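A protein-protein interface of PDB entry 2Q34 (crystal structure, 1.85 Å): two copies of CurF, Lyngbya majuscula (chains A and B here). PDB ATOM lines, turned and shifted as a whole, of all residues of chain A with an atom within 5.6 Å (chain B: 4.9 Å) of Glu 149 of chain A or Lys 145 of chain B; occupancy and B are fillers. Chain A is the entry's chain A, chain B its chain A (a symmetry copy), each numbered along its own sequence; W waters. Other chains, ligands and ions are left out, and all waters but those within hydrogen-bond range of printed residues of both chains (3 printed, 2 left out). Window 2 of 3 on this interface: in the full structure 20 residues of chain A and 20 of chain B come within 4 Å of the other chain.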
ATOM      1  N   GLY A 147     -10.287 -25.401  -9.744  1.00  0.00           N
ATOM      2  CA  GLY A 147      -8.887 -25.508  -9.350  1.00  0.00           C
ATOM      3  C   GLY A 147      -8.078 -24.426 -10.033  1.00  0.00           C
ATOM      4  O   GLY A 147      -8.391 -24.042 -11.173  1.00  0.00           O
ATOM      5  N   SER A 148      -7.041 -23.943  -9.345  1.00  0.00           N
ATOM      6  CA  SER A 148      -6.262 -22.783  -9.793  1.00  0.00           C
ATOM      7  C   SER A 148      -5.590 -22.969 -11.156  1.00  0.00           C
ATOM      8  O   SER A 148      -5.544 -22.028 -11.942  1.00  0.00           O
ATOM      9  CB  SER A 148      -5.236 -22.356  -8.733  1.00  0.00           C
ATOM     10  OG  SER A 148      -4.439 -23.456  -8.276  1.00  0.00           O
ATOM     11  N   GLU A 149      -5.091 -24.174 -11.438  1.00  0.00           N
ATOM     12  CA  GLU A 149      -4.323 -24.426 -12.674  1.00  0.00           C
ATOM     13  C   GLU A 149      -5.158 -24.447 -13.945  1.00  0.00           C
ATOM     14  O   GLU A 149      -4.815 -23.791 -14.926  1.00  0.00           O
ATOM     15  CB  GLU A 149      -3.510 -25.724 -12.566  1.00  0.00           C
ATOM     16  CG  GLU A 149      -2.083 -25.516 -12.106  1.00  0.00           C
ATOM     17  CD  GLU A 149      -1.941 -24.574 -10.901  1.00  0.00           C
ATOM     18  OE1 GLU A 149      -2.295 -24.996  -9.773  1.00  0.00           O
ATOM     19  OE2 GLU A 149      -1.454 -23.428 -11.086  1.00  0.00           O
ATOM     20  N   LEU A 150      -6.249 -25.204 -13.924  1.00  0.00           N
ATOM     21  CA  LEU A 150      -7.188 -25.193 -15.041  1.00  0.00           C
ATOM     22  C   LEU A 150      -7.773 -23.800 -15.188  1.00  0.00           C
ATOM     23  O   LEU A 150      -7.897 -23.308 -16.300  1.00  0.00           O
ATOM     24  CB  LEU A 150      -8.341 -26.185 -14.831  1.00  0.00           C
ATOM     25  CG  LEU A 150      -8.862 -27.065 -15.985  1.00  0.00           C
ATOM     26  CD1 LEU A 150     -10.293 -27.524 -15.712  1.00  0.00           C
ATOM     27  CD2 LEU A 150      -8.718 -26.507 -17.414  1.00  0.00           C
ATOM     28  N   ALA A 151      -8.150 -23.177 -14.073  1.00  0.00           N
ATOM     29  CA  ALA A 151      -8.726 -21.842 -14.134  1.00  0.00           C
ATOM     30  C   ALA A 151      -7.749 -20.908 -14.852  1.00  0.00           C
ATOM     31  O   ALA A 151      -8.129 -20.178 -15.762  1.00  0.00           O
ATOM     32  CB  ALA A 151      -9.052 -21.324 -12.730  1.00  0.00           C
ATOM     33  N   GLN A 152      -6.479 -20.971 -14.468  1.00  0.00           N
ATOM     34  CA  GLN A 152      -5.492 -20.059 -15.043  1.00  0.00           C
ATOM     35  C   GLN A 152      -5.306 -20.236 -16.557  1.00  0.00           C
ATOM     36  O   GLN A 152      -5.279 -19.254 -17.299  1.00  0.00           O
ATOM     37  CB  GLN A 152      -4.169 -20.200 -14.312  1.00  0.00           C
ATOM     38  CG  GLN A 152      -3.383 -18.930 -14.309  1.00  0.00           C
ATOM     39  CD  GLN A 152      -2.567 -18.777 -13.057  1.00  0.00           C
ATOM     40  OE1 GLN A 152      -3.109 -18.681 -11.956  1.00  0.00           O
ATOM     41  NE2 GLN A 152      -1.264 -18.764 -13.212  1.00  0.00           N
ATOM     42  N   GLU A 153      -5.203 -21.478 -17.015  1.00  0.00           N
ATOM     43  CA  GLU A 153      -5.084 -21.735 -18.439  1.00  0.00           C
ATOM     44  C   GLU A 153      -6.293 -21.226 -19.196  1.00  0.00           C
ATOM     45  O   GLU A 153      -6.156 -20.515 -20.180  1.00  0.00           O
ATOM     46  CB  GLU A 153      -4.901 -23.214 -18.731  1.00  0.00           C
ATOM     47  CG  GLU A 153      -4.471 -23.436 -20.172  1.00  0.00           C
ATOM     48  CD  GLU A 153      -4.384 -24.889 -20.499  1.00  0.00           C
ATOM     49  OE1 GLU A 153      -3.535 -25.564 -19.895  1.00  0.00           O
ATOM     50  OE2 GLU A 153      -5.169 -25.354 -21.346  1.00  0.00           O
ATOM     51  N   MET A 154      -7.481 -21.592 -18.732  1.00  0.00           N
ATOM     52  CA  MET A 154      -8.706 -21.117 -19.367  1.00  0.00           C
ATOM     53  C   MET A 154      -8.795 -19.599 -19.431  1.00  0.00           C
ATOM     54  O   MET A 154      -9.139 -19.050 -20.477  1.00  0.00           O
ATOM     55  CB  MET A 154      -9.928 -21.699 -18.655  1.00  0.00           C
ATOM     56  CG  MET A 154      -9.963 -23.197 -18.760  1.00  0.00           C
ATOM     57  SD  MET A 154     -11.710 -23.845 -18.121  1.00  0.00           S
ATOM     58  CE  MET A 154     -12.829 -23.191 -19.598  1.00  0.00           C
ATOM     59  N   LEU B 110       8.093 -23.997  -9.600  1.00  0.00           N
ATOM     60  CA  LEU B 110       6.727 -23.810  -9.112  1.00  0.00           C
ATOM     61  C   LEU B 110       6.358 -22.356  -8.825  1.00  0.00           C
ATOM     62  O   LEU B 110       5.165 -22.036  -8.666  1.00  0.00           O
ATOM     63  CB  LEU B 110       6.457 -24.690  -7.884  1.00  0.00           C
ATOM     64  CG  LEU B 110       6.388 -26.198  -8.193  1.00  0.00           C
ATOM     65  CD1 LEU B 110       6.240 -26.984  -6.889  1.00  0.00           C
ATOM     66  CD2 LEU B 110       5.299 -26.591  -9.184  1.00  0.00           C
ATOM     67  N   TYR B 111       7.347 -21.468  -8.775  1.00  0.00           N
ATOM     68  CA  TYR B 111       7.070 -20.014  -8.663  1.00  0.00           C
ATOM     69  C   TYR B 111       6.435 -19.465  -9.939  1.00  0.00           C
ATOM     70  O   TYR B 111       5.783 -18.388  -9.914  1.00  0.00           O
ATOM     71  CB  TYR B 111       8.352 -19.206  -8.386  1.00  0.00           C
ATOM     72  CG  TYR B 111       8.971 -19.367  -6.997  1.00  0.00           C
ATOM     73  CD1 TYR B 111       8.187 -19.657  -5.875  1.00  0.00           C
ATOM     74  CD2 TYR B 111      10.352 -19.219  -6.813  1.00  0.00           C
ATOM     75  CE1 TYR B 111       8.781 -19.803  -4.577  1.00  0.00           C
ATOM     76  CE2 TYR B 111      10.940 -19.354  -5.547  1.00  0.00           C
ATOM     77  CZ  TYR B 111      10.148 -19.648  -4.434  1.00  0.00           C
ATOM     78  OH  TYR B 111      10.754 -19.773  -3.177  1.00  0.00           O
ATOM     79  N   ALA B 112       6.643 -20.175 -11.046  1.00  0.00           N
ATOM     80  CA  ALA B 112       6.126 -19.760 -12.356  1.00  0.00           C
ATOM     81  C   ALA B 112       4.591 -19.855 -12.450  1.00  0.00           C
ATOM     82  O   ALA B 112       3.936 -20.511 -11.630  1.00  0.00           O
ATOM     83  CB  ALA B 112       6.771 -20.580 -13.457  1.00  0.00           C
ATOM     84  N   ASP B 113       4.029 -19.201 -13.461  1.00  0.00           N
ATOM     85  CA  ASP B 113       2.584 -19.197 -13.648  1.00  0.00           C
ATOM     86  C   ASP B 113       2.074 -20.529 -14.193  1.00  0.00           C
ATOM     87  O   ASP B 113       0.975 -20.974 -13.815  1.00  0.00           O
ATOM     88  CB  ASP B 113       2.211 -18.020 -14.540  1.00  0.00           C
ATOM     89  CG  ASP B 113       2.773 -16.714 -13.995  1.00  0.00           C
ATOM     90  OD1 ASP B 113       2.232 -16.192 -12.997  1.00  0.00           O
ATOM     91  OD2 ASP B 113       3.804 -16.250 -14.503  1.00  0.00           O
ATOM     92  N   ILE B 141       3.640 -22.521  -1.464  1.00  0.00           N
ATOM     93  CA  ILE B 141       3.649 -22.719  -2.907  1.00  0.00           C
ATOM     94  C   ILE B 141       3.238 -24.115  -3.293  1.00  0.00           C
ATOM     95  O   ILE B 141       2.380 -24.292  -4.154  1.00  0.00           O
ATOM     96  CB  ILE B 141       5.028 -22.388  -3.513  1.00  0.00           C
ATOM     97  CG1 ILE B 141       5.317 -20.892  -3.357  1.00  0.00           C
ATOM     98  CG2 ILE B 141       5.071 -22.783  -4.999  1.00  0.00           C
ATOM     99  CD1 ILE B 141       4.300 -19.958  -4.092  1.00  0.00           C
ATOM    100  N   LEU B 142       3.816 -25.117  -2.640  1.00  0.00           N
ATOM    101  CA  LEU B 142       3.504 -26.506  -3.011  1.00  0.00           C
ATOM    102  C   LEU B 142       2.053 -26.872  -2.753  1.00  0.00           C
ATOM    103  O   LEU B 142       1.431 -27.568  -3.562  1.00  0.00           O
ATOM    104  CB  LEU B 142       4.408 -27.482  -2.258  1.00  0.00           C
ATOM    105  CG  LEU B 142       5.477 -28.196  -3.068  1.00  0.00           C
ATOM    106  CD1 LEU B 142       6.609 -27.255  -3.381  1.00  0.00           C
ATOM    107  CD2 LEU B 142       5.938 -29.372  -2.220  1.00  0.00           C
ATOM    108  N   ARG B 143       1.515 -26.419  -1.627  1.00  0.00           N
ATOM    109  CA  ARG B 143       0.116 -26.663  -1.308  1.00  0.00           C
ATOM    110  C   ARG B 143      -0.822 -25.961  -2.276  1.00  0.00           C
ATOM    111  O   ARG B 143      -1.810 -26.553  -2.712  1.00  0.00           O
ATOM    112  CB  ARG B 143      -0.203 -26.308   0.145  1.00  0.00           C
ATOM    113  CG  ARG B 143       0.535 -27.231   1.109  1.00  0.00           C
ATOM    114  CD  ARG B 143      -0.164 -27.338   2.443  1.00  0.00           C
ATOM    115  NE  ARG B 143       0.114 -26.206   3.312  1.00  0.00           N
ATOM    116  CZ  ARG B 143      -0.243 -26.163   4.593  1.00  0.00           C
ATOM    117  NH1 ARG B 143      -0.885 -27.191   5.126  1.00  0.00           N
ATOM    118  NH2 ARG B 143       0.039 -25.101   5.336  1.00  0.00           N
ATOM    119  N   GLU B 144      -0.517 -24.711  -2.614  1.00  0.00           N
ATOM    120  CA  GLU B 144      -1.298 -23.993  -3.608  1.00  0.00           C
ATOM    121  C   GLU B 144      -1.249 -24.663  -4.992  1.00  0.00           C
ATOM    122  O   GLU B 144      -2.277 -24.782  -5.645  1.00  0.00           O
ATOM    123  CB  GLU B 144      -0.853 -22.523  -3.703  1.00  0.00           C
ATOM    124  CG  GLU B 144      -1.524 -21.713  -4.822  1.00  0.00           C
ATOM    125  CD  GLU B 144      -3.005 -21.409  -4.577  1.00  0.00           C
ATOM    126  OE1 GLU B 144      -3.547 -21.784  -3.504  1.00  0.00           O
ATOM    127  OE2 GLU B 144      -3.629 -20.770  -5.465  1.00  0.00           O
ATOM    128  N   LYS B 145      -0.081 -25.099  -5.444  1.00  0.00           N
ATOM    129  CA  LYS B 145       0.051 -25.546  -6.841  1.00  0.00           C
ATOM    130  C   LYS B 145      -0.215 -27.024  -7.018  1.00  0.00           C
ATOM    131  O   LYS B 145      -0.859 -27.421  -7.995  1.00  0.00           O
ATOM    132  CB  LYS B 145       1.430 -25.227  -7.403  1.00  0.00           C
ATOM    133  CG  LYS B 145       1.859 -23.777  -7.227  1.00  0.00           C
ATOM    134  CD  LYS B 145       1.584 -22.923  -8.421  1.00  0.00           C
ATOM    135  CE  LYS B 145       1.890 -21.470  -8.086  1.00  0.00           C
ATOM    136  NZ  LYS B 145       2.687 -20.846  -9.178  1.00  0.00           N
ATOM    137  N   LEU B 146       0.290 -27.837  -6.085  1.00  0.00           N
ATOM    138  CA  LEU B 146       0.191 -29.293  -6.194  1.00  0.00           C
ATOM    139  C   LEU B 146      -1.006 -29.862  -5.456  1.00  0.00           C
ATOM    140  O   LEU B 146      -1.338 -31.025  -5.649  1.00  0.00           O
ATOM    141  CB  LEU B 146       1.447 -29.977  -5.649  1.00  0.00           C
ATOM    142  CG  LEU B 146       2.808 -29.537  -6.168  1.00  0.00           C
ATOM    143  CD1 LEU B 146       3.912 -30.353  -5.512  1.00  0.00           C
ATOM    144  CD2 LEU B 146       2.856 -29.679  -7.669  1.00  0.00           C
ATOM    145  N   GLY B 147      -1.640 -29.064  -4.604  1.00  0.00           N
ATOM    146  CA  GLY B 147      -2.672 -29.587  -3.715  1.00  0.00           C
ATOM    147  C   GLY B 147      -2.052 -30.001  -2.398  1.00  0.00           C
ATOM    148  O   GLY B 147      -0.897 -30.459  -2.371  1.00  0.00           O
ATOM    149  N   PRO B 172      -2.006 -31.399 -10.832  1.00  0.00           N
ATOM    150  CA  PRO B 172      -2.798 -30.562 -11.748  1.00  0.00           C
ATOM    151  C   PRO B 172      -2.066 -29.998 -12.971  1.00  0.00           C
ATOM    152  O   PRO B 172      -2.616 -29.144 -13.684  1.00  0.00           O
ATOM    153  CB  PRO B 172      -3.273 -29.411 -10.850  1.00  0.00           C
ATOM    154  CG  PRO B 172      -2.956 -29.819  -9.449  1.00  0.00           C
ATOM    155  CD  PRO B 172      -1.762 -30.708  -9.554  1.00  0.00           C
ATOM    156  N   PHE B 173      -0.845 -30.456 -13.220  1.00  0.00           N
ATOM    157  CA  PHE B 173      -0.030 -29.925 -14.327  1.00  0.00           C
ATOM    158  C   PHE B 173       0.197 -30.972 -15.410  1.00  0.00           C
ATOM    159  O   PHE B 173       0.117 -32.169 -15.135  1.00  0.00           O
ATOM    160  CB  PHE B 173       1.334 -29.463 -13.799  1.00  0.00           C
ATOM    161  CG  PHE B 173       1.270 -28.263 -12.883  1.00  0.00           C
ATOM    162  CD1 PHE B 173       1.081 -26.993 -13.399  1.00  0.00           C
ATOM    163  CD2 PHE B 173       1.390 -28.416 -11.510  1.00  0.00           C
ATOM    164  CE1 PHE B 173       1.045 -25.865 -12.555  1.00  0.00           C
ATOM    165  CE2 PHE B 173       1.350 -27.312 -10.658  1.00  0.00           C
ATOM    166  CZ  PHE B 173       1.184 -26.035 -11.184  1.00  0.00           C
HETATM  167  O   HOH W   1       0.456 -20.855 -10.892  1.00  0.00           O
HETATM  168  O   HOH W   2      -0.702 -15.845 -13.219  1.00  0.00           O
HETATM  169  O   HOH W   3      -1.033 -22.988 -13.928  1.00  0.00           O
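Glu 149 of chain A touches just these residues of chain B: Lys 145 (3.3 Å), Pro 172 (3.7 Å) and Phe 173 (3.2 Å).
Of chain A, only Glu 149 comes within 4 Å of Lys 145 of chain B.
Printed residues of chain A within 4 Å of Glu 144 of chain B: Ser 148 (3.7 Å).
Printed residues of chain B within 4 Å of Ser 148 of chain A: Glu 144.
Of the printed residues of chain A, Asp 113 of chain B touches Gln 152 (3.2 Å).
Printed residues of chain A within 4 Å of Pro 172 of chain B: Glu 149.
Arg 143 of chain B touches none of the printed residues of chain A.
The nearest residue of chain B that does not touch Glu 149 of chain A is Glu 144 of chain B (4.1 Å).
The nearest residue of chain A that does not touch Lys 145 of chain B is Ser 148 of chain A (5.2 Å).
Water W1 lies within hydrogen-bond range of NZ of Lys 145 of chain B, O of Asp 113 of chain B and OE2 of Glu 149 of chain A.
Water W3 bridges O of Asp 113 of chain B (2.8 Å) and OE2 of Glu 149 of chain A (2.9 Å).
Water W2 lies within hydrogen-bond range of OD1 of Asp 113 of chain B (3.0 Å) and NE2 of Gln 152 of chain A (3.0 Å).
Ser 148 of chain A touches Glu 144 of chain B (OG to O, 3.7 Å).
CB of Glu 149 of chain A touches O of Pro 172 of chain B (3.7 Å).
Glu 149 of chain A touches Phe 173 of chain B.
Hydrophobic or aromatic side chains of chain B that line the printed part of chain A: Phe 173.
Of the 8 printed residues of chain A, 3 touch a printed residue of chain B.
Along chain A the printed residues that touch a printed residue of chain B span positions 148 to 152.
Among the printed residues, no Asp or Glu carboxylate lies within 4 Å of a Lys or Arg side-chain nitrogen of the other chain.
Position printed for both chains: 147.
Of the 5 pairs that touch across the chains among the printed residues, none has its exchanged pair printed and touching as well.
OE1 of Glu 149 of chain A lies within hydrogen-bond range of OG of Ser 148 of chain A (3.0 Å).
The backbone carbonyl oxygen (O) of Leu 110 of chain B lies within hydrogen-bond range of the side-chain amino group (NZ) of Lys 145 of chain B (2.8 Å).
The side-chain amino group (NZ) of Lys 145 of chain B is in hydrogen-bond range of the backbone carbonyl oxygen (O) of Ala 112 of chain B, 2.8 Å away.
NE2 of Gln 152 of chain A sits at hydrogen-bond distance from O of Asp 113 of chain B, 3.2 Å away.
The backbone carbonyl oxygen of Lys 145 of chain B lies close to the side-chain carboxylate of Glu 149 of chain A (3.3 Å).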
